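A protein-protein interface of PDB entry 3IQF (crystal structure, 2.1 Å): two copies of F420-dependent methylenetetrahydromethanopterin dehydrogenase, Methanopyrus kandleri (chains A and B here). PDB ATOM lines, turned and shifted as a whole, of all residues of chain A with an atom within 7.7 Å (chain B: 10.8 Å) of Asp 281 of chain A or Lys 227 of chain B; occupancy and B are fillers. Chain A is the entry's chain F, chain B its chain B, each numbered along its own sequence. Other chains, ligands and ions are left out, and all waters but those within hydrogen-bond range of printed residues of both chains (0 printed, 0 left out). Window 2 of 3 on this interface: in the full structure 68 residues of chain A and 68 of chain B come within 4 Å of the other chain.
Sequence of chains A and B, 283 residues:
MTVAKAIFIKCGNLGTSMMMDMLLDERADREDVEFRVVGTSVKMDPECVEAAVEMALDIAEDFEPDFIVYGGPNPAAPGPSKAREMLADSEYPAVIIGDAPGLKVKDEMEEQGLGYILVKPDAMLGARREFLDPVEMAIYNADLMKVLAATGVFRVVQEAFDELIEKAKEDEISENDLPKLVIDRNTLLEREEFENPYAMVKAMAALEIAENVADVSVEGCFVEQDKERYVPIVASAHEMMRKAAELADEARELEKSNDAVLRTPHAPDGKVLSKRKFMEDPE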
ATOM      1  N   PRO A 265     -20.889 -11.669   0.798  1.00  0.00           N
ATOM      2  CA  PRO A 265     -21.073 -12.113   2.168  1.00  0.00           C
ATOM      3  C   PRO A 265     -22.493 -12.441   2.486  1.00  0.00           C
ATOM      4  O   PRO A 265     -23.427 -11.926   1.816  1.00  0.00           O
ATOM      5  CB  PRO A 265     -20.648 -10.897   2.990  1.00  0.00           C
ATOM      6  CG  PRO A 265     -21.019  -9.711   2.101  1.00  0.00           C
ATOM      7  CD  PRO A 265     -20.706 -10.199   0.700  1.00  0.00           C
ATOM      8  N   LEU A 273     -25.355 -11.382   0.018  1.00  0.00           N
ATOM      9  CA  LEU A 273     -25.244  -9.997  -0.430  1.00  0.00           C
ATOM     10  C   LEU A 273     -24.180  -9.949  -1.504  1.00  0.00           C
ATOM     11  O   LEU A 273     -23.551 -10.968  -1.788  1.00  0.00           O
ATOM     12  CB  LEU A 273     -24.915  -9.058   0.726  1.00  0.00           C
ATOM     13  CG  LEU A 273     -25.850  -9.246   1.956  1.00  0.00           C
ATOM     14  CD1 LEU A 273     -25.236  -8.689   3.214  1.00  0.00           C
ATOM     15  CD2 LEU A 273     -27.229  -8.624   1.674  1.00  0.00           C
ATOM     16  N   SER A 274     -24.000  -8.759  -2.089  1.00  0.00           N
ATOM     17  CA  SER A 274     -23.052  -8.551  -3.164  1.00  0.00           C
ATOM     18  C   SER A 274     -22.462  -7.151  -3.096  1.00  0.00           C
ATOM     19  O   SER A 274     -23.165  -6.175  -2.782  1.00  0.00           O
ATOM     20  CB  SER A 274     -23.776  -8.692  -4.502  1.00  0.00           C
ATOM     21  OG  SER A 274     -22.953  -9.345  -5.407  1.00  0.00           O
ATOM     22  N   LYS A 275     -21.197  -7.054  -3.477  1.00  0.00           N
ATOM     23  CA  LYS A 275     -20.550  -5.762  -3.731  1.00  0.00           C
ATOM     24  C   LYS A 275     -19.335  -5.935  -4.653  1.00  0.00           C
ATOM     25  O   LYS A 275     -18.820  -7.042  -4.820  1.00  0.00           O
ATOM     26  CB  LYS A 275     -20.138  -5.122  -2.386  1.00  0.00           C
ATOM     27  CG  LYS A 275     -19.229  -6.022  -1.511  1.00  0.00           C
ATOM     28  CD  LYS A 275     -18.724  -5.318  -0.283  1.00  0.00           C
ATOM     29  CE  LYS A 275     -17.601  -4.307  -0.606  1.00  0.00           C
ATOM     30  NZ  LYS A 275     -17.309  -3.451   0.620  1.00  0.00           N
ATOM     31  N   ARG A 276     -18.891  -4.824  -5.245  1.00  0.00           N
ATOM     32  CA  ARG A 276     -17.620  -4.748  -5.958  1.00  0.00           C
ATOM     33  C   ARG A 276     -16.675  -3.636  -5.454  1.00  0.00           C
ATOM     34  O   ARG A 276     -15.480  -3.826  -5.404  1.00  0.00           O
ATOM     35  CB  ARG A 276     -17.844  -4.588  -7.458  1.00  0.00           C
ATOM     36  CG  ARG A 276     -17.889  -5.933  -8.189  1.00  0.00           C
ATOM     37  CD  ARG A 276     -17.586  -5.761  -9.608  1.00  0.00           C
ATOM     38  NE  ARG A 276     -18.011  -6.948 -10.318  1.00  0.00           N
ATOM     39  CZ  ARG A 276     -17.309  -8.060 -10.418  1.00  0.00           C
ATOM     40  NH1 ARG A 276     -17.829  -9.074 -11.076  1.00  0.00           N
ATOM     41  NH2 ARG A 276     -16.110  -8.169  -9.871  1.00  0.00           N
ATOM     42  N   LYS A 277     -17.196  -2.460  -5.129  1.00  0.00           N
ATOM     43  CA  LYS A 277     -16.324  -1.364  -4.670  1.00  0.00           C
ATOM     44  C   LYS A 277     -15.951  -1.595  -3.221  1.00  0.00           C
ATOM     45  O   LYS A 277     -16.774  -2.069  -2.449  1.00  0.00           O
ATOM     46  CB  LYS A 277     -17.027  -0.008  -4.818  1.00  0.00           C
ATOM     47  CG  LYS A 277     -17.537   0.236  -6.255  1.00  0.00           C
ATOM     48  CD  LYS A 277     -16.523   1.032  -7.086  1.00  0.00           C
ATOM     49  CE  LYS A 277     -16.735   2.587  -6.811  1.00  0.00           C
ATOM     50  NZ  LYS A 277     -18.114   3.126  -7.167  1.00  0.00           N
ATOM     51  N   PHE A 278     -14.709  -1.273  -2.873  1.00  0.00           N
ATOM     52  CA  PHE A 278     -14.200  -1.506  -1.533  1.00  0.00           C
ATOM     53  C   PHE A 278     -15.109  -0.880  -0.467  1.00  0.00           C
ATOM     54  O   PHE A 278     -15.458  -1.534   0.514  1.00  0.00           O
ATOM     55  CB  PHE A 278     -12.768  -0.952  -1.407  1.00  0.00           C
ATOM     56  CG  PHE A 278     -12.125  -1.213  -0.057  1.00  0.00           C
ATOM     57  CD1 PHE A 278     -11.991  -0.182   0.885  1.00  0.00           C
ATOM     58  CD2 PHE A 278     -11.699  -2.485   0.289  1.00  0.00           C
ATOM     59  CE1 PHE A 278     -11.412  -0.428   2.147  1.00  0.00           C
ATOM     60  CE2 PHE A 278     -11.117  -2.739   1.530  1.00  0.00           C
ATOM     61  CZ  PHE A 278     -10.966  -1.702   2.455  1.00  0.00           C
ATOM     62  N   MET A 279     -15.481   0.385  -0.661  1.00  0.00           N
ATOM     63  CA  MET A 279     -16.279   1.107   0.315  1.00  0.00           C
ATOM     64  C   MET A 279     -17.808   1.010   0.097  1.00  0.00           C
ATOM     65  O   MET A 279     -18.572   1.586   0.838  1.00  0.00           O
ATOM     66  CB  MET A 279     -15.812   2.577   0.349  1.00  0.00           C
ATOM     67  CG  MET A 279     -14.503   2.791   1.165  1.00  0.00           C
ATOM     68  SD  MET A 279     -14.398   1.705   2.593  1.00  0.00           S
ATOM     69  CE  MET A 279     -15.515   2.426   3.779  1.00  0.00           C
ATOM     70  N   GLU A 280     -18.245   0.257  -0.912  1.00  0.00           N
ATOM     71  CA  GLU A 280     -19.686  -0.014  -1.136  1.00  0.00           C
ATOM     72  C   GLU A 280     -20.190  -1.024  -0.096  1.00  0.00           C
ATOM     73  O   GLU A 280     -19.542  -2.053   0.112  1.00  0.00           O
ATOM     74  CB  GLU A 280     -19.869  -0.566  -2.591  1.00  0.00           C
ATOM     75  CG  GLU A 280     -21.171  -1.356  -2.962  1.00  0.00           C
ATOM     76  CD  GLU A 280     -21.142  -2.039  -4.379  1.00  0.00           C
ATOM     77  OE1 GLU A 280     -20.094  -2.135  -5.034  1.00  0.00           O
ATOM     78  OE2 GLU A 280     -22.203  -2.499  -4.858  1.00  0.00           O
ATOM     79  N   ASP A 281     -21.304  -0.720   0.564  1.00  0.00           N
ATOM     80  CA  ASP A 281     -21.955  -1.673   1.468  1.00  0.00           C
ATOM     81  C   ASP A 281     -22.543  -2.868   0.712  1.00  0.00           C
ATOM     82  O   ASP A 281     -23.126  -2.705  -0.346  1.00  0.00           O
ATOM     83  CB  ASP A 281     -22.993  -0.973   2.347  1.00  0.00           C
ATOM     84  CG  ASP A 281     -22.328  -0.189   3.482  1.00  0.00           C
ATOM     85  OD1 ASP A 281     -21.162  -0.521   3.866  1.00  0.00           O
ATOM     86  OD2 ASP A 281     -22.939   0.766   3.962  1.00  0.00           O
ATOM     87  N   PRO A 282     -22.353  -4.087   1.244  1.00  0.00           N
ATOM     88  CA  PRO A 282     -22.874  -5.232   0.511  1.00  0.00           C
ATOM     89  C   PRO A 282     -24.368  -5.248   0.594  1.00  0.00           C
ATOM     90  O   PRO A 282     -24.882  -5.016   1.648  1.00  0.00           O
ATOM     91  CB  PRO A 282     -22.255  -6.455   1.242  1.00  0.00           C
ATOM     92  CG  PRO A 282     -21.882  -5.976   2.590  1.00  0.00           C
ATOM     93  CD  PRO A 282     -21.677  -4.468   2.498  1.00  0.00           C
ATOM     94  N   GLU A 283     -25.059  -5.494  -0.517  1.00  0.00           N
ATOM     95  CA  GLU A 283     -26.530  -5.508  -0.524  1.00  0.00           C
ATOM     96  C   GLU A 283     -27.119  -6.599  -1.433  1.00  0.00           C
ATOM     97  O   GLU A 283     -28.306  -6.944  -1.352  1.00  0.00           O
ATOM     98  CB  GLU A 283     -27.091  -4.106  -0.872  1.00  0.00           C
ATOM     99  CG  GLU A 283     -26.244  -2.973  -0.247  1.00  0.00           C
ATOM    100  CD  GLU A 283     -27.032  -1.909   0.432  1.00  0.00           C
ATOM    101  OE1 GLU A 283     -27.042  -1.876   1.706  1.00  0.00           O
ATOM    102  OE2 GLU A 283     -27.614  -1.106  -0.321  1.00  0.00           O
ATOM    103  OXT GLU A 283     -26.445  -7.189  -2.253  1.00  0.00           O
ATOM    104  N   ARG B 128     -15.397  -8.433   9.381  1.00  0.00           N
ATOM    105  CA  ARG B 128     -16.467  -7.458   9.179  1.00  0.00           C
ATOM    106  C   ARG B 128     -17.153  -7.757   7.856  1.00  0.00           C
ATOM    107  O   ARG B 128     -16.487  -8.014   6.833  1.00  0.00           O
ATOM    108  CB  ARG B 128     -15.894  -6.042   9.135  1.00  0.00           C
ATOM    109  CG  ARG B 128     -15.337  -5.502  10.436  1.00  0.00           C
ATOM    110  CD  ARG B 128     -16.432  -5.273  11.501  1.00  0.00           C
ATOM    111  NE  ARG B 128     -15.971  -4.328  12.524  1.00  0.00           N
ATOM    112  CZ  ARG B 128     -16.772  -3.636  13.330  1.00  0.00           C
ATOM    113  NH1 ARG B 128     -16.238  -2.810  14.207  1.00  0.00           N
ATOM    114  NH2 ARG B 128     -18.089  -3.782  13.280  1.00  0.00           N
ATOM    115  N   ARG B 129     -18.474  -7.716   7.871  1.00  0.00           N
ATOM    116  CA  ARG B 129     -19.289  -8.119   6.694  1.00  0.00           C
ATOM    117  C   ARG B 129     -18.956  -7.415   5.382  1.00  0.00           C
ATOM    118  O   ARG B 129     -19.071  -8.009   4.297  1.00  0.00           O
ATOM    119  CB  ARG B 129     -20.759  -7.903   6.988  1.00  0.00           C
ATOM    120  CG  ARG B 129     -21.652  -8.548   5.905  1.00  0.00           C
ATOM    121  CD  ARG B 129     -23.093  -8.497   6.286  1.00  0.00           C
ATOM    122  NE  ARG B 129     -23.323  -9.244   7.517  1.00  0.00           N
ATOM    123  CZ  ARG B 129     -23.714  -8.701   8.668  1.00  0.00           C
ATOM    124  NH1 ARG B 129     -23.854  -9.477   9.717  1.00  0.00           N
ATOM    125  NH2 ARG B 129     -23.942  -7.395   8.779  1.00  0.00           N
ATOM    126  N   GLU B 130     -18.525  -6.160   5.489  1.00  0.00           N
ATOM    127  CA  GLU B 130     -18.255  -5.330   4.332  1.00  0.00           C
ATOM    128  C   GLU B 130     -17.020  -5.786   3.592  1.00  0.00           C
ATOM    129  O   GLU B 130     -16.819  -5.465   2.422  1.00  0.00           O
ATOM    130  CB  GLU B 130     -18.075  -3.848   4.758  1.00  0.00           C
ATOM    131  CG  GLU B 130     -19.268  -3.225   5.474  1.00  0.00           C
ATOM    132  CD  GLU B 130     -19.206  -3.353   6.986  1.00  0.00           C
ATOM    133  OE1 GLU B 130     -19.858  -2.524   7.641  1.00  0.00           O
ATOM    134  OE2 GLU B 130     -18.537  -4.289   7.516  1.00  0.00           O
ATOM    135  N   PHE B 131     -16.178  -6.544   4.298  1.00  0.00           N
ATOM    136  CA  PHE B 131     -14.921  -7.011   3.783  1.00  0.00           C
ATOM    137  C   PHE B 131     -14.854  -8.547   3.661  1.00  0.00           C
ATOM    138  O   PHE B 131     -14.450  -9.069   2.658  1.00  0.00           O
ATOM    139  CB  PHE B 131     -13.810  -6.519   4.716  1.00  0.00           C
ATOM    140  CG  PHE B 131     -12.451  -6.966   4.283  1.00  0.00           C
ATOM    141  CD1 PHE B 131     -11.913  -6.493   3.091  1.00  0.00           C
ATOM    142  CD2 PHE B 131     -11.744  -7.889   5.025  1.00  0.00           C
ATOM    143  CE1 PHE B 131     -10.693  -6.925   2.653  1.00  0.00           C
ATOM    144  CE2 PHE B 131     -10.538  -8.371   4.566  1.00  0.00           C
ATOM    145  CZ  PHE B 131     -10.005  -7.883   3.378  1.00  0.00           C
ATOM    146  N   LEU B 132     -15.214  -9.249   4.714  1.00  0.00           N
ATOM    147  CA  LEU B 132     -15.006 -10.691   4.780  1.00  0.00           C
ATOM    148  C   LEU B 132     -16.182 -11.484   4.223  1.00  0.00           C
ATOM    149  O   LEU B 132     -17.195 -11.697   4.906  1.00  0.00           O
ATOM    150  CB  LEU B 132     -14.756 -11.155   6.223  1.00  0.00           C
ATOM    151  CG  LEU B 132     -14.085 -12.545   6.297  1.00  0.00           C
ATOM    152  CD1 LEU B 132     -12.610 -12.431   6.085  1.00  0.00           C
ATOM    153  CD2 LEU B 132     -14.354 -13.288   7.544  1.00  0.00           C
ATOM    154  N   GLU B 219      -8.578  -4.443  16.553  1.00  0.00           N
ATOM    155  CA  GLU B 219      -8.931  -3.019  16.486  1.00  0.00           C
ATOM    156  C   GLU B 219     -10.070  -2.836  15.506  1.00  0.00           C
ATOM    157  O   GLU B 219     -11.050  -2.154  15.775  1.00  0.00           O
ATOM    158  CB  GLU B 219      -7.735  -2.156  16.047  1.00  0.00           C
ATOM    159  CG  GLU B 219      -8.064  -0.636  15.938  1.00  0.00           C
ATOM    160  CD  GLU B 219      -6.875   0.214  15.376  1.00  0.00           C
ATOM    161  OE1 GLU B 219      -5.716  -0.151  15.608  1.00  0.00           O
ATOM    162  OE2 GLU B 219      -7.119   1.258  14.719  1.00  0.00           O
ATOM    163  N   GLY B 220      -9.953  -3.469  14.353  1.00  0.00           N
ATOM    164  CA  GLY B 220     -10.963  -3.287  13.318  1.00  0.00           C
ATOM    165  C   GLY B 220     -12.311  -3.903  13.646  1.00  0.00           C
ATOM    166  O   GLY B 220     -13.346  -3.356  13.259  1.00  0.00           O
ATOM    167  N   CYS B 221     -12.301  -5.034  14.330  1.00  0.00           N
ATOM    168  CA  CYS B 221     -13.557  -5.769  14.601  1.00  0.00           C
ATOM    169  C   CYS B 221     -14.226  -5.394  15.927  1.00  0.00           C
ATOM    170  O   CYS B 221     -15.431  -5.517  16.024  1.00  0.00           O
ATOM    171  CB  CYS B 221     -13.352  -7.272  14.621  1.00  0.00           C
ATOM    172  SG  CYS B 221     -12.934  -7.997  13.038  1.00  0.00           S
ATOM    173  N   VAL B 223     -13.011  -2.533  18.243  1.00  0.00           N
ATOM    174  CA  VAL B 223     -12.749  -1.227  18.879  1.00  0.00           C
ATOM    175  C   VAL B 223     -13.289  -0.119  18.014  1.00  0.00           C
ATOM    176  O   VAL B 223     -14.142   0.656  18.456  1.00  0.00           O
ATOM    177  CB  VAL B 223     -11.246  -1.031  19.174  1.00  0.00           C
ATOM    178  CG1 VAL B 223     -11.003   0.325  19.856  1.00  0.00           C
ATOM    179  CG2 VAL B 223     -10.744  -2.185  20.039  1.00  0.00           C
ATOM    180  N   GLU B 224     -12.806  -0.076  16.770  1.00  0.00           N
ATOM    181  CA  GLU B 224     -13.245   0.930  15.827  1.00  0.00           C
ATOM    182  C   GLU B 224     -14.685   0.646  15.436  1.00  0.00           C
ATOM    183  O   GLU B 224     -15.018  -0.469  15.024  1.00  0.00           O
ATOM    184  CB  GLU B 224     -12.357   0.919  14.562  1.00  0.00           C
ATOM    185  CG  GLU B 224     -12.804   1.929  13.520  1.00  0.00           C
ATOM    186  CD  GLU B 224     -12.717   3.358  14.007  1.00  0.00           C
ATOM    187  OE1 GLU B 224     -13.756   4.045  14.005  1.00  0.00           O
ATOM    188  OE2 GLU B 224     -11.599   3.775  14.377  1.00  0.00           O
ATOM    189  N   GLN B 225     -15.518   1.676  15.514  1.00  0.00           N
ATOM    190  CA  GLN B 225     -16.941   1.555  15.251  1.00  0.00           C
ATOM    191  C   GLN B 225     -17.402   2.288  13.978  1.00  0.00           C
ATOM    192  O   GLN B 225     -18.524   2.090  13.566  1.00  0.00           O
ATOM    193  CB  GLN B 225     -17.741   2.062  16.475  1.00  0.00           C
ATOM    194  CG  GLN B 225     -17.528   1.203  17.765  1.00  0.00           C
ATOM    195  CD  GLN B 225     -18.102  -0.230  17.615  1.00  0.00           C
ATOM    196  OE1 GLN B 225     -19.323  -0.398  17.485  1.00  0.00           O
ATOM    197  NE2 GLN B 225     -17.234  -1.250  17.660  1.00  0.00           N
ATOM    198  N   ASP B 226     -16.550   3.110  13.367  1.00  0.00           N
ATOM    199  CA  ASP B 226     -16.887   3.813  12.094  1.00  0.00           C
ATOM    200  C   ASP B 226     -16.415   2.977  10.899  1.00  0.00           C
ATOM    201  O   ASP B 226     -15.215   2.751  10.754  1.00  0.00           O
ATOM    202  CB  ASP B 226     -16.243   5.219  12.099  1.00  0.00           C
ATOM    203  CG  ASP B 226     -16.420   6.013  10.763  1.00  0.00           C
ATOM    204  OD1 ASP B 226     -15.926   7.179  10.732  1.00  0.00           O
ATOM    205  OD2 ASP B 226     -17.009   5.506   9.762  1.00  0.00           O
ATOM    206  N   LYS B 227     -17.342   2.533  10.039  1.00  0.00           N
ATOM    207  CA  LYS B 227     -16.977   1.683   8.894  1.00  0.00           C
ATOM    208  C   LYS B 227     -16.007   2.308   7.914  1.00  0.00           C
ATOM    209  O   LYS B 227     -15.211   1.586   7.301  1.00  0.00           O
ATOM    210  CB  LYS B 227     -18.170   1.102   8.116  1.00  0.00           C
ATOM    211  CG  LYS B 227     -19.082   2.078   7.460  1.00  0.00           C
ATOM    212  CD  LYS B 227     -20.094   1.323   6.568  1.00  0.00           C
ATOM    213  CE  LYS B 227     -21.498   1.932   6.616  1.00  0.00           C
ATOM    214  NZ  LYS B 227     -21.708   3.191   5.845  1.00  0.00           N
ATOM    215  N   GLU B 228     -16.036   3.636   7.779  1.00  0.00           N
ATOM    216  CA  GLU B 228     -15.063   4.313   6.909  1.00  0.00           C
ATOM    217  C   GLU B 228     -13.653   4.121   7.456  1.00  0.00           C
ATOM    218  O   GLU B 228     -12.700   4.261   6.728  1.00  0.00           O
ATOM    219  CB  GLU B 228     -15.359   5.822   6.711  1.00  0.00           C
ATOM    220  CG  GLU B 228     -16.521   6.117   5.772  1.00  0.00           C
ATOM    221  CD  GLU B 228     -16.817   7.606   5.672  1.00  0.00           C
ATOM    222  OE1 GLU B 228     -17.820   8.063   6.285  1.00  0.00           O
ATOM    223  OE2 GLU B 228     -16.045   8.333   4.978  1.00  0.00           O
ATOM    224  N   ARG B 229     -13.539   3.809   8.748  1.00  0.00           N
ATOM    225  CA  ARG B 229     -12.253   3.462   9.335  1.00  0.00           C
ATOM    226  C   ARG B 229     -12.061   1.965   9.439  1.00  0.00           C
ATOM    227  O   ARG B 229     -10.986   1.469   9.111  1.00  0.00           O
ATOM    228  CB  ARG B 229     -12.048   4.150  10.676  1.00  0.00           C
ATOM    229  CG  ARG B 229     -11.881   5.689  10.554  1.00  0.00           C
ATOM    230  CD  ARG B 229     -11.893   6.348  11.930  1.00  0.00           C
ATOM    231  NE  ARG B 229     -10.638   6.088  12.630  1.00  0.00           N
ATOM    232  CZ  ARG B 229      -9.540   6.841  12.538  1.00  0.00           C
ATOM    233  NH1 ARG B 229      -8.487   6.494  13.247  1.00  0.00           N
ATOM    234  NH2 ARG B 229      -9.468   7.921  11.748  1.00  0.00           N
ATOM    235  N   TYR B 230     -13.067   1.220   9.898  1.00  0.00           N
ATOM    236  CA  TYR B 230     -12.794  -0.189  10.195  1.00  0.00           C
ATOM    237  C   TYR B 230     -12.648  -1.065   8.991  1.00  0.00           C
ATOM    238  O   TYR B 230     -11.963  -2.076   9.060  1.00  0.00           O
ATOM    239  CB  TYR B 230     -13.749  -0.789  11.242  1.00  0.00           C
ATOM    240  CG  TYR B 230     -15.190  -0.980  10.899  1.00  0.00           C
ATOM    241  CD1 TYR B 230     -16.184  -0.337  11.636  1.00  0.00           C
ATOM    242  CD2 TYR B 230     -15.582  -1.881   9.932  1.00  0.00           C
ATOM    243  CE1 TYR B 230     -17.553  -0.531  11.356  1.00  0.00           C
ATOM    244  CE2 TYR B 230     -16.958  -2.065   9.626  1.00  0.00           C
ATOM    245  CZ  TYR B 230     -17.922  -1.410  10.354  1.00  0.00           C
ATOM    246  OH  TYR B 230     -19.250  -1.608  10.050  1.00  0.00           O
ATOM    247  N   VAL B 231     -13.279  -0.711   7.877  1.00  0.00           N
ATOM    248  CA  VAL B 231     -13.125  -1.558   6.656  1.00  0.00           C
ATOM    249  C   VAL B 231     -11.668  -1.505   6.133  1.00  0.00           C
ATOM    250  O   VAL B 231     -11.019  -2.536   5.949  1.00  0.00           O
ATOM    251  CB  VAL B 231     -14.192  -1.217   5.597  1.00  0.00           C
ATOM    252  CG1 VAL B 231     -14.041  -2.040   4.365  1.00  0.00           C
ATOM    253  CG2 VAL B 231     -15.579  -1.451   6.200  1.00  0.00           C
ATOM    254  N   PRO B 232     -11.132  -0.304   5.958  1.00  0.00           N
ATOM    255  CA  PRO B 232      -9.717  -0.215   5.655  1.00  0.00           C
ATOM    256  C   PRO B 232      -8.777  -0.878   6.663  1.00  0.00           C
ATOM    257  O   PRO B 232      -7.845  -1.560   6.282  1.00  0.00           O
ATOM    258  CB  PRO B 232      -9.464   1.307   5.550  1.00  0.00           C
ATOM    259  CG  PRO B 232     -10.740   1.959   5.551  1.00  0.00           C
ATOM    260  CD  PRO B 232     -11.812   1.002   5.921  1.00  0.00           C
ATOM    261  N   ILE B 233      -9.078  -0.741   7.954  1.00  0.00           N
ATOM    262  CA  ILE B 233      -8.278  -1.410   8.982  1.00  0.00           C
ATOM    263  C   ILE B 233      -8.249  -2.952   8.830  1.00  0.00           C
ATOM    264  O   ILE B 233      -7.153  -3.578   8.783  1.00  0.00           O
ATOM    265  CB  ILE B 233      -8.712  -0.986  10.426  1.00  0.00           C
ATOM    266  CG1 ILE B 233      -8.315   0.468  10.715  1.00  0.00           C
ATOM    267  CG2 ILE B 233      -8.036  -1.860  11.474  1.00  0.00           C
ATOM    268  CD1 ILE B 233      -8.964   1.063  12.051  1.00  0.00           C
ATOM    269  N   VAL B 234      -9.421  -3.584   8.755  1.00  0.00           N
ATOM    270  CA  VAL B 234      -9.418  -5.056   8.604  1.00  0.00           C
ATOM    271  C   VAL B 234      -8.771  -5.503   7.288  1.00  0.00           C
ATOM    272  O   VAL B 234      -8.068  -6.528   7.244  1.00  0.00           O
ATOM    273  CB  VAL B 234     -10.803  -5.732   8.822  1.00  0.00           C
ATOM    274  CG1 VAL B 234     -11.331  -5.455  10.246  1.00  0.00           C
ATOM    275  CG2 VAL B 234     -11.822  -5.334   7.770  1.00  0.00           C
ATOM    276  N   ALA B 235      -9.004  -4.744   6.204  1.00  0.00           N
ATOM    277  CA  ALA B 235      -8.394  -5.049   4.942  1.00  0.00           C
ATOM    278  C   ALA B 235      -6.854  -4.986   5.017  1.00  0.00           C
ATOM    279  O   ALA B 235      -6.160  -5.792   4.433  1.00  0.00           O
ATOM    280  CB  ALA B 235      -8.938  -4.146   3.885  1.00  0.00           C
ATOM    281  N   SER B 236      -6.326  -4.034   5.778  1.00  0.00           N
ATOM    282  CA  SER B 236      -4.913  -3.905   5.927  1.00  0.00           C
ATOM    283  C   SER B 236      -4.278  -5.107   6.660  1.00  0.00           C
ATOM    284  O   SER B 236      -3.144  -5.477   6.380  1.00  0.00           O
ATOM    285  CB  SER B 236      -4.574  -2.543   6.564  1.00  0.00           C
ATOM    286  OG  SER B 236      -4.708  -2.512   7.943  1.00  0.00           O
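O of Glu 130 of chain B sits at hydrogen-bond distance from NZ of Lys 275 of chain A, at 2.7 Å. NZ of Lys 227 of chain B lies within salt-bridge range of OD2 of Asp 281 of chain A.
CG of Pro 265 of chain A touches O of Arg 129 of chain B, at 3.4 Å. CD of Arg 129 of chain B touches CD1 of Leu 273 of chain A, at 3.8 Å. Phe 278 of chain A touches Val 231 of chain B (CZ to O, 3.6 Å). Pro 232 of chain B touches Phe 278 of chain A. Ala 235 of chain B touches Phe 278 of chain A (CB to CZ, 3.5 Å). O of Lys 227 of chain B touches CE of Met 279 of chain A, 3.6 Å away. Glu 228 of chain B touches Met 279 of chain A. CG of Glu 130 of chain B touches OD1 of Asp 281 of chain A (3.7 Å). Arg 129 of chain B touches Pro 282 of chain A. Glu 130 of chain B touches Pro 282 of chain A (CA to CD, 3.98 Å).
No position is printed for both chains. Of the 12 pairs that touch across the chains among the printed residues, none has its exchanged pair printed and touching as well.
The side-chain carboxylate (OE1) of Glu 130 of chain B lies within hydrogen-bond range of the side-chain hydroxyl (OH) of Tyr 230 of chain B. The side-chain carboxylate (OD2) of Asp 226 of chain B sits at hydrogen-bond distance from the backbone NH (N) of Glu 228 of chain B (2.9 Å). O of Pro 265 of chain A is in hydrogen-bond range of N of Leu 273 of chain A, at 2.7 Å. NZ of Lys 275 of chain A sits close to O of Lys 277 of chain A. O of Phe 278 of chain A lies within hydrogen-bond range of NZ of Lys 275 of chain A, 2.7 Å away. The side-chain amino group of Lys 275 of chain A sits at hydrogen-bond distance from the backbone carbonyl oxygen of Glu 280 of chain A (2.7 Å).
Hydrophobic or aromatic side chains of chain A within 4 Å of the printed part of chain B: Pro 265, Leu 273, Phe 278, Met 279 and Pro 282. Hydrophobic or aromatic side chains of chain B within 4 Å of the printed part of chain A: Val 231 and Ala 235. Among the printed residues, 12 pairs touch across the chains. Among the printed residues, Asp or Glu carboxylates within 4 Å of a Lys or Arg side-chain nitrogen of the other chain: Asp 281 of chain A with Lys 227 of chain B (3.3 Å).
Of the printed residues of chain B, Lys 275 of chain A touches Glu 130 (2.7 Å). Lys 277 of chain A touches none of the printed residues of chain B. Of chain B, only Glu 130 (3.7 Å) and Lys 227 (3.2 Å) come within 4 Å of Asp 281 of chain A. Of the printed residues of chain A, Glu 130 of chain B touches Lys 275 (2.7 Å), Asp 281 (3.7 Å) and Pro 282 (3.98 Å). Lys 227 of chain B touches just these residues of chain A: Met 279 and Asp 281. Arg 229 of chain B touches none of the printed residues of chain A. The nearest residue of chain A that does not touch Lys 227 of chain B is Phe 278 of chain A (6.7 Å). The nearest printed residue of chain B that does not touch Phe 278 of chain A is Phe 131 of chain B (4.1 Å).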
